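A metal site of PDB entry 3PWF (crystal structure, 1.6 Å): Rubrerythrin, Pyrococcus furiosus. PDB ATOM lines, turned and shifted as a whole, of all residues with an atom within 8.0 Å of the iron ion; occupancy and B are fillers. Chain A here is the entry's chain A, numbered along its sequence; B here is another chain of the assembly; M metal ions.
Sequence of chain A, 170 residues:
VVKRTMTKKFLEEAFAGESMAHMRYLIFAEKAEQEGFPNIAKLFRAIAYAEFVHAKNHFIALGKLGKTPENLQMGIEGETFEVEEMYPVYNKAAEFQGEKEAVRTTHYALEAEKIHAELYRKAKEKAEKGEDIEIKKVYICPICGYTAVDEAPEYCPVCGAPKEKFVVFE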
ATOM      1  N   TYR A 108      -9.495 -14.226 -20.521  1.00  0.00           N
ATOM      2  CA  TYR A 108      -8.767 -15.446 -20.804  1.00  0.00           C
ATOM      3  C   TYR A 108      -9.651 -16.550 -21.305  1.00  0.00           C
ATOM      4  O   TYR A 108      -9.415 -17.261 -22.325  1.00  0.00           O
ATOM      5  CB  TYR A 108      -8.040 -15.950 -19.535  1.00  0.00           C
ATOM      6  CG  TYR A 108      -6.825 -15.168 -19.132  1.00  0.00           C
ATOM      7  CD1 TYR A 108      -6.373 -14.117 -19.858  1.00  0.00           C
ATOM      8  CD2 TYR A 108      -6.146 -15.533 -17.988  1.00  0.00           C
ATOM      9  CE1 TYR A 108      -5.176 -13.440 -19.482  1.00  0.00           C
ATOM     10  CE2 TYR A 108      -4.953 -14.880 -17.590  1.00  0.00           C
ATOM     11  CZ  TYR A 108      -4.488 -13.887 -18.408  1.00  0.00           C
ATOM     12  OH  TYR A 108      -3.311 -13.176 -17.941  1.00  0.00           O
ATOM     13  N   ILE A 140      -1.782 -26.552 -24.704  1.00  0.00           N
ATOM     14  CA  ILE A 140      -2.645 -25.702 -23.874  1.00  0.00           C
ATOM     15  C   ILE A 140      -1.815 -24.790 -22.953  1.00  0.00           C
ATOM     16  O   ILE A 140      -1.009 -25.234 -22.142  1.00  0.00           O
ATOM     17  CB  ILE A 140      -3.585 -26.577 -22.976  1.00  0.00           C
ATOM     18  CG1 ILE A 140      -4.363 -27.667 -23.783  1.00  0.00           C
ATOM     19  CG2 ILE A 140      -4.512 -25.632 -22.227  1.00  0.00           C
ATOM     20  CD1 ILE A 140      -5.407 -27.125 -24.825  1.00  0.00           C
ATOM     21  N   CYS A 141      -2.076 -23.484 -23.052  1.00  0.00           N
ATOM     22  CA  CYS A 141      -1.435 -22.530 -22.115  1.00  0.00           C
ATOM     23  C   CYS A 141      -1.933 -22.728 -20.685  1.00  0.00           C
ATOM     24  O   CYS A 141      -3.196 -22.751 -20.460  1.00  0.00           O
ATOM     25  CB  CYS A 141      -1.699 -21.051 -22.554  1.00  0.00           C
ATOM     26  SG  CYS A 141      -0.929 -19.879 -21.380  1.00  0.00           S
ATOM     27  N   PRO A 142      -1.069 -22.985 -19.720  1.00  0.00           N
ATOM     28  CA  PRO A 142      -1.522 -23.213 -18.348  1.00  0.00           C
ATOM     29  C   PRO A 142      -1.937 -21.997 -17.589  1.00  0.00           C
ATOM     30  O   PRO A 142      -2.495 -22.143 -16.447  1.00  0.00           O
ATOM     31  CB  PRO A 142      -0.258 -23.858 -17.674  1.00  0.00           C
ATOM     32  CG  PRO A 142       0.874 -23.096 -18.372  1.00  0.00           C
ATOM     33  CD  PRO A 142       0.423 -23.119 -19.853  1.00  0.00           C
ATOM     34  N   ILE A 143      -1.739 -20.819 -18.181  1.00  0.00           N
ATOM     35  CA  ILE A 143      -2.187 -19.555 -17.538  1.00  0.00           C
ATOM     36  C   ILE A 143      -3.633 -19.176 -17.986  1.00  0.00           C
ATOM     37  O   ILE A 143      -4.470 -18.737 -17.163  1.00  0.00           O
ATOM     38  CB  ILE A 143      -1.228 -18.490 -17.919  1.00  0.00           C
ATOM     39  CG1 ILE A 143       0.251 -18.925 -17.538  1.00  0.00           C
ATOM     40  CG2 ILE A 143      -1.604 -17.202 -17.305  1.00  0.00           C
ATOM     41  CD1 ILE A 143       0.380 -19.301 -16.102  1.00  0.00           C
ATOM     42  N   CYS A 144      -3.909 -19.268 -19.285  1.00  0.00           N
ATOM     43  CA  CYS A 144      -5.146 -18.707 -19.842  1.00  0.00           C
ATOM     44  C   CYS A 144      -5.928 -19.738 -20.586  1.00  0.00           C
ATOM     45  O   CYS A 144      -7.133 -19.449 -20.979  1.00  0.00           O
ATOM     46  CB  CYS A 144      -4.978 -17.435 -20.690  1.00  0.00           C
ATOM     47  SG  CYS A 144      -4.121 -17.852 -22.263  1.00  0.00           S
ATOM     48  N   GLY A 145      -5.366 -20.931 -20.869  1.00  0.00           N
ATOM     49  CA  GLY A 145      -6.159 -21.898 -21.616  1.00  0.00           C
ATOM     50  C   GLY A 145      -6.208 -21.722 -23.129  1.00  0.00           C
ATOM     51  O   GLY A 145      -6.866 -22.489 -23.808  1.00  0.00           O
ATOM     52  N   TYR A 146      -5.382 -20.796 -23.635  1.00  0.00           N
ATOM     53  CA  TYR A 146      -5.155 -20.717 -25.084  1.00  0.00           C
ATOM     54  C   TYR A 146      -4.826 -22.096 -25.590  1.00  0.00           C
ATOM     55  O   TYR A 146      -4.068 -22.858 -24.966  1.00  0.00           O
ATOM     56  CB  TYR A 146      -3.954 -19.718 -25.373  1.00  0.00           C
ATOM     57  CG  TYR A 146      -3.469 -19.802 -26.833  1.00  0.00           C
ATOM     58  CD1 TYR A 146      -2.282 -20.526 -27.085  1.00  0.00           C
ATOM     59  CD2 TYR A 146      -4.196 -19.235 -27.881  1.00  0.00           C
ATOM     60  CE1 TYR A 146      -1.831 -20.668 -28.374  1.00  0.00           C
ATOM     61  CE2 TYR A 146      -3.761 -19.338 -29.151  1.00  0.00           C
ATOM     62  CZ  TYR A 146      -2.546 -20.037 -29.378  1.00  0.00           C
ATOM     63  OH  TYR A 146      -2.131 -20.180 -30.707  1.00  0.00           O
ATOM     64  N   THR A 147      -5.374 -22.426 -26.768  1.00  0.00           N
ATOM     65  CA  THR A 147      -5.348 -23.813 -27.269  1.00  0.00           C
ATOM     66  C   THR A 147      -4.869 -23.736 -28.732  1.00  0.00           C
ATOM     67  O   THR A 147      -5.378 -22.953 -29.570  1.00  0.00           O
ATOM     68  CB  THR A 147      -6.773 -24.340 -27.256  1.00  0.00           C
ATOM     69  OG1 THR A 147      -7.244 -24.403 -25.892  1.00  0.00           O
ATOM     70  CG2 THR A 147      -6.905 -25.746 -27.860  1.00  0.00           C
ATOM     71  N   TYR A 155       5.065 -17.599 -28.119  1.00  0.00           N
ATOM     72  CA  TYR A 155       4.550 -16.980 -26.917  1.00  0.00           C
ATOM     73  C   TYR A 155       3.017 -16.967 -27.094  1.00  0.00           C
ATOM     74  O   TYR A 155       2.472 -16.799 -28.168  1.00  0.00           O
ATOM     75  CB  TYR A 155       5.027 -15.541 -26.804  1.00  0.00           C
ATOM     76  CG  TYR A 155       6.553 -15.486 -26.554  1.00  0.00           C
ATOM     77  CD1 TYR A 155       7.054 -15.803 -25.287  1.00  0.00           C
ATOM     78  CD2 TYR A 155       7.380 -15.337 -27.639  1.00  0.00           C
ATOM     79  CE1 TYR A 155       8.439 -15.883 -25.078  1.00  0.00           C
ATOM     80  CE2 TYR A 155       8.813 -15.368 -27.411  1.00  0.00           C
ATOM     81  CZ  TYR A 155       9.260 -15.655 -26.139  1.00  0.00           C
ATOM     82  OH  TYR A 155      10.647 -15.738 -25.976  1.00  0.00           O
ATOM     83  N   CYS A 156       2.324 -17.250 -25.949  1.00  0.00           N
ATOM     84  CA  CYS A 156       0.859 -17.223 -25.966  1.00  0.00           C
ATOM     85  C   CYS A 156       0.400 -15.816 -26.395  1.00  0.00           C
ATOM     86  O   CYS A 156       0.808 -14.786 -25.845  1.00  0.00           O
ATOM     87  CB  CYS A 156       0.492 -17.489 -24.530  1.00  0.00           C
ATOM     88  SG  CYS A 156      -1.455 -17.385 -24.451  1.00  0.00           S
ATOM     89  N   PRO A 157      -0.572 -15.757 -27.351  1.00  0.00           N
ATOM     90  CA  PRO A 157      -0.957 -14.393 -27.824  1.00  0.00           C
ATOM     91  C   PRO A 157      -1.886 -13.663 -26.844  1.00  0.00           C
ATOM     92  O   PRO A 157      -2.075 -12.439 -26.962  1.00  0.00           O
ATOM     93  CB  PRO A 157      -1.682 -14.663 -29.157  1.00  0.00           C
ATOM     94  CG  PRO A 157      -2.220 -16.066 -28.967  1.00  0.00           C
ATOM     95  CD  PRO A 157      -1.087 -16.835 -28.181  1.00  0.00           C
ATOM     96  N   VAL A 158      -2.350 -14.422 -25.826  1.00  0.00           N
ATOM     97  CA  VAL A 158      -3.262 -13.757 -24.880  1.00  0.00           C
ATOM     98  C   VAL A 158      -2.502 -13.297 -23.693  1.00  0.00           C
ATOM     99  O   VAL A 158      -2.690 -12.100 -23.297  1.00  0.00           O
ATOM    100  CB  VAL A 158      -4.439 -14.761 -24.509  1.00  0.00           C
ATOM    101  CG1 VAL A 158      -5.240 -14.065 -23.326  1.00  0.00           C
ATOM    102  CG2 VAL A 158      -5.299 -15.086 -25.716  1.00  0.00           C
ATOM    103  N   CYS A 159      -1.667 -14.146 -23.110  1.00  0.00           N
ATOM    104  CA  CYS A 159      -0.998 -13.723 -21.869  1.00  0.00           C
ATOM    105  C   CYS A 159       0.505 -13.651 -21.980  1.00  0.00           C
ATOM    106  O   CYS A 159       1.171 -13.237 -21.010  1.00  0.00           O
ATOM    107  CB  CYS A 159      -1.381 -14.716 -20.745  1.00  0.00           C
ATOM    108  SG  CYS A 159      -0.611 -16.374 -20.885  1.00  0.00           S
ATOM    109  N   GLY A 160       1.062 -14.036 -23.126  1.00  0.00           N
ATOM    110  CA  GLY A 160       2.503 -13.958 -23.384  1.00  0.00           C
ATOM    111  C   GLY A 160       3.377 -15.048 -22.754  1.00  0.00           C
ATOM    112  O   GLY A 160       4.621 -15.023 -22.869  1.00  0.00           O
ATOM    113  N   ALA A 161       2.792 -16.050 -22.107  1.00  0.00           N
ATOM    114  CA  ALA A 161       3.592 -17.211 -21.605  1.00  0.00           C
ATOM    115  C   ALA A 161       4.352 -17.875 -22.721  1.00  0.00           C
ATOM    116  O   ALA A 161       3.885 -18.079 -23.852  1.00  0.00           O
ATOM    117  CB  ALA A 161       2.645 -18.367 -21.005  1.00  0.00           C
ATOM    118  N   PRO A 162       5.577 -18.340 -22.397  1.00  0.00           N
ATOM    119  CA  PRO A 162       6.408 -18.973 -23.430  1.00  0.00           C
ATOM    120  C   PRO A 162       5.882 -20.354 -23.722  1.00  0.00           C
ATOM    121  O   PRO A 162       5.421 -21.127 -22.850  1.00  0.00           O
ATOM    122  CB  PRO A 162       7.795 -19.087 -22.740  1.00  0.00           C
ATOM    123  CG  PRO A 162       7.535 -19.041 -21.270  1.00  0.00           C
ATOM    124  CD  PRO A 162       6.248 -18.172 -21.086  1.00  0.00           C
ATOM    125  N   PHE A 166       3.713 -24.540 -22.224  1.00  0.00           N
ATOM    126  CA  PHE A 166       2.421 -25.143 -22.661  1.00  0.00           C
ATOM    127  C   PHE A 166       2.342 -26.617 -22.351  1.00  0.00           C
ATOM    128  O   PHE A 166       3.371 -27.411 -22.462  1.00  0.00           O
ATOM    129  CB  PHE A 166       2.173 -24.964 -24.163  1.00  0.00           C
ATOM    130  CG  PHE A 166       2.098 -23.510 -24.636  1.00  0.00           C
ATOM    131  CD1 PHE A 166       2.041 -22.432 -23.759  1.00  0.00           C
ATOM    132  CD2 PHE A 166       2.138 -23.293 -26.008  1.00  0.00           C
ATOM    133  CE1 PHE A 166       1.943 -21.100 -24.205  1.00  0.00           C
ATOM    134  CE2 PHE A 166       2.067 -21.923 -26.559  1.00  0.00           C
ATOM    135  CZ  PHE A 166       1.940 -20.807 -25.662  1.00  0.00           C
ATOM    136  N   VAL B  53      -8.006 -24.922 -16.518  1.00  0.00           N
ATOM    137  CA  VAL B  53      -7.355 -23.693 -16.350  1.00  0.00           C
ATOM    138  C   VAL B  53      -8.351 -22.524 -16.110  1.00  0.00           C
ATOM    139  O   VAL B  53      -8.174 -21.723 -15.185  1.00  0.00           O
ATOM    140  CB  VAL B  53      -6.439 -23.304 -17.529  1.00  0.00           C
ATOM    141  CG1 VAL B  53      -5.840 -21.919 -17.444  1.00  0.00           C
ATOM    142  CG2 VAL B  53      -5.310 -24.392 -17.731  1.00  0.00           C
HETATM  143 FE    FE M   1      -1.805 -17.858 -22.200  1.00  0.00          FE
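The backbone NH (N) of Ala 161 lies close to the side-chain sulfur (SG) of Cys 159 (3.6 Å). SG of Cys 144 sits close to N of Tyr 146, 3.5 Å away. The backbone NH of Cys 156 is in hydrogen-bond range of the backbone carbonyl oxygen of Ala 161 (2.7 Å). The side-chain sulfur (SG) of Cys 156 sits close to the backbone NH (N) of Val 158. N of Cys 141 lies within hydrogen-bond range of O of Tyr 146 (2.8 Å). The backbone NH (N) of Ile 143 lies close to the side-chain sulfur (SG) of Cys 141 (3.4 Å).
The iron ion is bound by the side-chain sulfur (SG) of Cys 159 (2.3 Å). SG of Cys 144 is bound to the iron ion. SG of Cys 156 is bound to the iron ion (2.3 Å). The iron ion is bound by SG of Cys 141, 2.4 Å away. The iron ion has four donor atoms within binding distance.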
